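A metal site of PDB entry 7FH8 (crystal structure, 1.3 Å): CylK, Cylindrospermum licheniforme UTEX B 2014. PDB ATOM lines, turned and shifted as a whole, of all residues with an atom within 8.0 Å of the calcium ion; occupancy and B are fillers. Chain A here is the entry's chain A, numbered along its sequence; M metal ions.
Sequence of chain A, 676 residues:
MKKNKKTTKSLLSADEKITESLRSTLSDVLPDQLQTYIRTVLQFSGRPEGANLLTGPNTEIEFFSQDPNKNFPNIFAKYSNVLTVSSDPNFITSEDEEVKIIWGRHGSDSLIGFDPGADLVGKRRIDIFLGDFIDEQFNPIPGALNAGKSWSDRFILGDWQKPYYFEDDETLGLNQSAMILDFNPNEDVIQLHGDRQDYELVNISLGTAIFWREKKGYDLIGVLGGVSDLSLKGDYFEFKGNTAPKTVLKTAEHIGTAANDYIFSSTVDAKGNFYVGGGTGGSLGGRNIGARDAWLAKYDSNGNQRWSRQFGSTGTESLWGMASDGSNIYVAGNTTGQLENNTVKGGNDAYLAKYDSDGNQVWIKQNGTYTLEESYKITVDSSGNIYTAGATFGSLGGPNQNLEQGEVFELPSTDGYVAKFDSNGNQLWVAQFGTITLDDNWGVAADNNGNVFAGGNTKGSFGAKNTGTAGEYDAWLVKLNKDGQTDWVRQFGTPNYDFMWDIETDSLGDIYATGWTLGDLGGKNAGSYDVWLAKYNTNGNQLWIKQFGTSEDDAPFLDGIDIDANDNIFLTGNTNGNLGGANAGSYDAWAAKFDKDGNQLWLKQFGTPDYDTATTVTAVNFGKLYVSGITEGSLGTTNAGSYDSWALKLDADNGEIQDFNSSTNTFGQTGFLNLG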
ATOM      1  N   PRO A  68      24.147  14.257  -7.123  1.00  0.00           N
ATOM      2  CA  PRO A  68      24.615  15.605  -6.762  1.00  0.00           C
ATOM      3  C   PRO A  68      24.486  16.613  -7.882  1.00  0.00           C
ATOM      4  O   PRO A  68      24.365  17.813  -7.597  1.00  0.00           O
ATOM      5  CB  PRO A  68      26.088  15.389  -6.368  1.00  0.00           C
ATOM      6  CG  PRO A  68      26.254  13.914  -6.177  1.00  0.00           C
ATOM      7  CD  PRO A  68      25.197  13.225  -6.990  1.00  0.00           C
ATOM      8  N   ASN A  74      21.626  21.618  -4.205  1.00  0.00           N
ATOM      9  CA  ASN A  74      22.964  21.876  -4.749  1.00  0.00           C
ATOM     10  C   ASN A  74      22.921  22.930  -5.846  1.00  0.00           C
ATOM     11  O   ASN A  74      23.754  23.843  -5.864  1.00  0.00           O
ATOM     12  CB  ASN A  74      23.584  20.597  -5.304  1.00  0.00           C
ATOM     13  CG  ASN A  74      24.016  19.619  -4.232  1.00  0.00           C
ATOM     14  OD1 ASN A  74      24.079  19.955  -3.043  1.00  0.00           O
ATOM     15  ND2 ASN A  74      24.359  18.411  -4.666  1.00  0.00           N
ATOM     16  N   THR A 335      33.417  23.722   2.006  1.00  0.00           N
ATOM     17  CA  THR A 335      34.065  23.879   0.717  1.00  0.00           C
ATOM     18  C   THR A 335      33.061  23.532  -0.377  1.00  0.00           C
ATOM     19  O   THR A 335      32.164  22.713  -0.177  1.00  0.00           O
ATOM     20  CB  THR A 335      35.336  23.011   0.583  1.00  0.00           C
ATOM     21  OG1 THR A 335      35.947  23.253  -0.689  1.00  0.00           O
ATOM     22  CG2 THR A 335      35.024  21.523   0.701  1.00  0.00           C
ATOM     23  N   VAL A 344      35.314  14.461  -2.937  1.00  0.00           N
ATOM     24  CA  VAL A 344      34.059  15.181  -2.768  1.00  0.00           C
ATOM     25  C   VAL A 344      32.926  14.198  -2.507  1.00  0.00           C
ATOM     26  O   VAL A 344      32.886  13.101  -3.082  1.00  0.00           O
ATOM     27  CB  VAL A 344      33.754  16.043  -4.004  1.00  0.00           C
ATOM     28  CG1 VAL A 344      34.814  17.091  -4.186  1.00  0.00           C
ATOM     29  CG2 VAL A 344      33.649  15.182  -5.251  1.00  0.00           C
ATOM     30  N   LYS A 345      31.989  14.592  -1.646  1.00  0.00           N
ATOM     31  CA  LYS A 345      30.809  13.779  -1.395  1.00  0.00           C
ATOM     32  C   LYS A 345      29.595  14.257  -2.175  1.00  0.00           C
ATOM     33  O   LYS A 345      28.651  13.483  -2.375  1.00  0.00           O
ATOM     34  CB  LYS A 345      30.469  13.719   0.108  1.00  0.00           C
ATOM     35  CG  LYS A 345      31.304  12.700   0.873  1.00  0.00           C
ATOM     36  CD  LYS A 345      32.731  13.173   1.030  1.00  0.00           C
ATOM     37  CE  LYS A 345      33.550  12.220   1.874  1.00  0.00           C
ATOM     38  NZ  LYS A 345      34.989  12.370   1.551  1.00  0.00           N
ATOM     39  N   GLY A 346      29.614  15.506  -2.636  1.00  0.00           N
ATOM     40  CA  GLY A 346      28.560  16.028  -3.487  1.00  0.00           C
ATOM     41  C   GLY A 346      28.143  17.422  -3.075  1.00  0.00           C
ATOM     42  O   GLY A 346      27.924  17.688  -1.885  1.00  0.00           O
ATOM     43  N   GLY A 347      28.051  18.339  -4.035  1.00  0.00           N
ATOM     44  CA  GLY A 347      27.735  19.702  -3.665  1.00  0.00           C
ATOM     45  C   GLY A 347      28.742  20.250  -2.672  1.00  0.00           C
ATOM     46  O   GLY A 347      29.928  19.903  -2.702  1.00  0.00           O
ATOM     47  N   ASN A 348      28.275  21.109  -1.778  1.00  0.00           N
ATOM     48  CA  ASN A 348      29.145  21.632  -0.734  1.00  0.00           C
ATOM     49  C   ASN A 348      29.313  20.599   0.368  1.00  0.00           C
ATOM     50  O   ASN A 348      28.360  19.896   0.716  1.00  0.00           O
ATOM     51  CB  ASN A 348      28.539  22.892  -0.110  1.00  0.00           C
ATOM     52  CG  ASN A 348      28.480  24.048  -1.075  1.00  0.00           C
ATOM     53  OD1 ASN A 348      28.844  23.932  -2.248  1.00  0.00           O
ATOM     54  ND2 ASN A 348      28.023  25.186  -0.581  1.00  0.00           N
ATOM     55  N   ASP A 349      30.513  20.530   0.926  1.00  0.00           N
ATOM     56  CA  ASP A 349      30.835  19.590   1.990  1.00  0.00           C
ATOM     57  C   ASP A 349      31.406  20.378   3.168  1.00  0.00           C
ATOM     58  O   ASP A 349      31.791  21.542   3.037  1.00  0.00           O
ATOM     59  CB  ASP A 349      31.917  18.596   1.550  1.00  0.00           C
ATOM     60  CG  ASP A 349      31.392  17.515   0.605  1.00  0.00           C
ATOM     61  OD1 ASP A 349      30.161  17.290   0.524  1.00  0.00           O
ATOM     62  OD2 ASP A 349      32.246  16.892  -0.062  1.00  0.00           O
ATOM     63  N   ALA A 350      31.431  19.727   4.326  1.00  0.00           N
ATOM     64  CA  ALA A 350      32.116  20.266   5.497  1.00  0.00           C
ATOM     65  C   ALA A 350      33.551  19.745   5.528  1.00  0.00           C
ATOM     66  O   ALA A 350      33.903  18.770   4.861  1.00  0.00           O
ATOM     67  CB  ALA A 350      31.388  19.858   6.778  1.00  0.00           C
ATOM     68  N   GLN A 366      37.472  15.904   4.737  1.00  0.00           N
ATOM     69  CA  GLN A 366      36.279  16.436   4.097  1.00  0.00           C
ATOM     70  C   GLN A 366      35.145  15.421   4.277  1.00  0.00           C
ATOM     71  O   GLN A 366      35.332  14.231   3.999  1.00  0.00           O
ATOM     72  CB  GLN A 366      36.549  16.659   2.605  1.00  0.00           C
ATOM     73  CG  GLN A 366      35.423  17.345   1.843  1.00  0.00           C
ATOM     74  CD  GLN A 366      35.882  17.841   0.486  1.00  0.00           C
ATOM     75  OE1 GLN A 366      37.084  18.098   0.280  1.00  0.00           O
ATOM     76  NE2 GLN A 366      34.937  17.998  -0.439  1.00  0.00           N
ATOM     77  N   ASN A 367      33.996  15.892   4.760  1.00  0.00           N
ATOM     78  CA  ASN A 367      32.902  14.970   5.069  1.00  0.00           C
ATOM     79  C   ASN A 367      31.578  15.574   4.631  1.00  0.00           C
ATOM     80  O   ASN A 367      31.436  16.790   4.556  1.00  0.00           O
ATOM     81  CB  ASN A 367      32.852  14.581   6.581  1.00  0.00           C
ATOM     82  CG  ASN A 367      32.362  15.725   7.496  1.00  0.00           C
ATOM     83  OD1 ASN A 367      32.983  16.770   7.603  1.00  0.00           O
ATOM     84  ND2 ASN A 367      31.240  15.482   8.185  1.00  0.00           N
ATOM     85  N   GLY A 368      30.617  14.709   4.338  1.00  0.00           N
ATOM     86  CA  GLY A 368      29.293  15.195   3.974  1.00  0.00           C
ATOM     87  C   GLY A 368      28.481  14.147   3.239  1.00  0.00           C
ATOM     88  O   GLY A 368      28.774  12.949   3.305  1.00  0.00           O
ATOM     89  N   THR A 369      27.443  14.629   2.568  1.00  0.00           N
ATOM     90  CA  THR A 369      26.522  13.835   1.776  1.00  0.00           C
ATOM     91  C   THR A 369      26.502  14.349   0.342  1.00  0.00           C
ATOM     92  O   THR A 369      27.167  15.338   0.002  1.00  0.00           O
ATOM     93  CB  THR A 369      25.097  13.904   2.334  1.00  0.00           C
ATOM     94  OG1 THR A 369      24.517  15.178   2.013  1.00  0.00           O
ATOM     95  CG2 THR A 369      25.080  13.702   3.857  1.00  0.00           C
ATOM     96  N   TYR A 370      25.705  13.683  -0.491  1.00  0.00           N
ATOM     97  CA  TYR A 370      25.498  14.078  -1.875  1.00  0.00           C
ATOM     98  C   TYR A 370      24.955  15.503  -2.019  1.00  0.00           C
ATOM     99  O   TYR A 370      25.044  16.080  -3.109  1.00  0.00           O
ATOM    100  CB  TYR A 370      24.514  13.110  -2.541  1.00  0.00           C
ATOM    101  CG  TYR A 370      23.143  13.130  -1.876  1.00  0.00           C
ATOM    102  CD1 TYR A 370      22.872  12.326  -0.782  1.00  0.00           C
ATOM    103  CD2 TYR A 370      22.130  13.964  -2.335  1.00  0.00           C
ATOM    104  CE1 TYR A 370      21.634  12.340  -0.157  1.00  0.00           C
ATOM    105  CE2 TYR A 370      20.886  13.990  -1.715  1.00  0.00           C
ATOM    106  CZ  TYR A 370      20.649  13.181  -0.630  1.00  0.00           C
ATOM    107  OH  TYR A 370      19.419  13.193   0.002  1.00  0.00           O
ATOM    108  N   THR A 371      24.358  16.061  -0.960  1.00  0.00           N
ATOM    109  CA  THR A 371      23.753  17.387  -1.033  1.00  0.00           C
ATOM    110  C   THR A 371      24.478  18.369  -0.103  1.00  0.00           C
ATOM    111  O   THR A 371      25.611  18.120   0.318  1.00  0.00           O
ATOM    112  CB  THR A 371      22.227  17.311  -0.835  1.00  0.00           C
ATOM    113  OG1 THR A 371      21.625  18.610  -0.947  1.00  0.00           O
ATOM    114  CG2 THR A 371      21.864  16.691   0.507  1.00  0.00           C
ATOM    115  N   LEU A 372      23.864  19.519   0.190  1.00  0.00           N
ATOM    116  CA  LEU A 372      24.598  20.597   0.852  1.00  0.00           C
ATOM    117  C   LEU A 372      24.836  20.329   2.340  1.00  0.00           C
ATOM    118  O   LEU A 372      23.887  20.035   3.083  1.00  0.00           O
ATOM    119  CB  LEU A 372      23.876  21.930   0.668  1.00  0.00           C
ATOM    120  CG  LEU A 372      24.601  23.157   1.260  1.00  0.00           C
ATOM    121  CD1 LEU A 372      24.367  24.361   0.389  1.00  0.00           C
ATOM    122  CD2 LEU A 372      24.142  23.477   2.690  1.00  0.00           C
ATOM    123  N   GLU A 373      26.091  20.478   2.761  1.00  0.00           N
ATOM    124  CA  GLU A 373      26.448  20.668   4.163  1.00  0.00           C
ATOM    125  C   GLU A 373      26.988  22.075   4.330  1.00  0.00           C
ATOM    126  O   GLU A 373      27.619  22.635   3.429  1.00  0.00           O
ATOM    127  CB  GLU A 373      27.558  19.708   4.621  1.00  0.00           C
ATOM    128  CG  GLU A 373      27.079  18.301   4.908  1.00  0.00           C
ATOM    129  CD  GLU A 373      26.662  17.557   3.652  1.00  0.00           C
ATOM    130  OE1 GLU A 373      27.490  17.471   2.719  1.00  0.00           O
ATOM    131  OE2 GLU A 373      25.517  17.072   3.608  1.00  0.00           O
ATOM    132  N   GLU A 374      26.742  22.651   5.509  1.00  0.00           N
ATOM    133  CA  GLU A 374      27.453  23.821   5.967  1.00  0.00           C
ATOM    134  C   GLU A 374      27.949  23.533   7.382  1.00  0.00           C
ATOM    135  O   GLU A 374      27.396  22.676   8.081  1.00  0.00           O
ATOM    136  CB  GLU A 374      26.592  25.091   5.931  1.00  0.00           C
ATOM    137  CG  GLU A 374      25.300  24.987   6.702  1.00  0.00           C
ATOM    138  CD  GLU A 374      24.463  26.249   6.593  1.00  0.00           C
ATOM    139  OE1 GLU A 374      24.529  26.908   5.533  1.00  0.00           O
ATOM    140  OE2 GLU A 374      23.735  26.572   7.554  1.00  0.00           O
ATOM    141  N   THR A 392      22.772  20.026   7.427  1.00  0.00           N
ATOM    142  CA  THR A 392      22.811  19.209   6.230  1.00  0.00           C
ATOM    143  C   THR A 392      21.425  19.045   5.633  1.00  0.00           C
ATOM    144  O   THR A 392      20.445  18.838   6.357  1.00  0.00           O
ATOM    145  CB  THR A 392      23.438  17.829   6.518  1.00  0.00           C
ATOM    146  OG1 THR A 392      23.460  17.045   5.317  1.00  0.00           O
ATOM    147  CG2 THR A 392      22.677  17.058   7.607  1.00  0.00           C
ATOM    148  N   PHE A 393      21.351  19.110   4.305  1.00  0.00           N
ATOM    149  CA  PHE A 393      20.144  18.739   3.584  1.00  0.00           C
ATOM    150  C   PHE A 393      20.038  17.231   3.374  1.00  0.00           C
ATOM    151  O   PHE A 393      19.045  16.763   2.801  1.00  0.00           O
ATOM    152  CB  PHE A 393      20.120  19.410   2.208  1.00  0.00           C
ATOM    153  CG  PHE A 393      19.715  20.848   2.246  1.00  0.00           C
ATOM    154  CD1 PHE A 393      20.656  21.842   2.489  1.00  0.00           C
ATOM    155  CD2 PHE A 393      18.400  21.220   1.992  1.00  0.00           C
ATOM    156  CE1 PHE A 393      20.293  23.175   2.502  1.00  0.00           C
ATOM    157  CE2 PHE A 393      18.029  22.555   1.998  1.00  0.00           C
ATOM    158  CZ  PHE A 393      18.976  23.536   2.261  1.00  0.00           C
ATOM    159  N   GLY A 394      21.045  16.463   3.783  1.00  0.00           N
ATOM    160  CA  GLY A 394      21.072  15.051   3.530  1.00  0.00           C
ATOM    161  C   GLY A 394      20.911  14.226   4.782  1.00  0.00           C
ATOM    162  O   GLY A 394      20.409  14.700   5.824  1.00  0.00           O
ATOM    163  N   LEU A 396      23.201  12.541   7.077  1.00  0.00           N
ATOM    164  CA  LEU A 396      24.600  12.457   7.479  1.00  0.00           C
ATOM    165  C   LEU A 396      24.767  11.622   8.750  1.00  0.00           C
ATOM    166  O   LEU A 396      25.530  10.664   8.763  1.00  0.00           O
ATOM    167  CB  LEU A 396      25.170  13.868   7.659  1.00  0.00           C
ATOM    168  CG  LEU A 396      26.666  13.995   7.936  1.00  0.00           C
ATOM    169  CD1 LEU A 396      27.476  13.520   6.730  1.00  0.00           C
ATOM    170  CD2 LEU A 396      27.002  15.425   8.281  1.00  0.00           C
HETATM  171 CA    CA M   1      27.867  17.584   0.388  1.00  0.00          CA
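The side-chain hydroxyl (OG1) of Thr 369 lies close to the backbone NH (N) of Thr 371 (3.1 Å).
OD1 of Asn 74 sits close to OG1 of Thr 371 (3.5 Å).
The backbone NH (N) of Lys 345 is in hydrogen-bond range of the side-chain carboxylate (OD2) of Asp 349 (2.8 Å).
OD2 of Asp 349 lies within hydrogen-bond range of NE2 of Gln 366, 2.9 Å away.
The side-chain carboxylate (OE2) of Glu 373 sits at hydrogen-bond distance from the side-chain hydroxyl (OG1) of Thr 392, 2.7 Å away.
O of Asp 349 lies within hydrogen-bond range of N of Thr 335 (2.9 Å).
Of the 23 residues printed, 6 come within 4 Å of the calcium ion.
Along chain A the residues within 4 Å of the calcium ion span positions 346 to 373.
The nearest printed residue that does not touch the calcium ion is Gly 347 (4.2 Å).
The calcium ion is bound by O of Gly 346 (2.3 Å).
The calcium ion is bound by OD1 of Asp 349.
The calcium ion is bound by O of Thr 371 (2.3 Å).
The calcium ion is bound by OE1 of Glu 373 (2.4 Å).
The backbone carbonyl oxygen (O) of Thr 369 binds the calcium ion.
O of Asn 348 binds the calcium ion.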
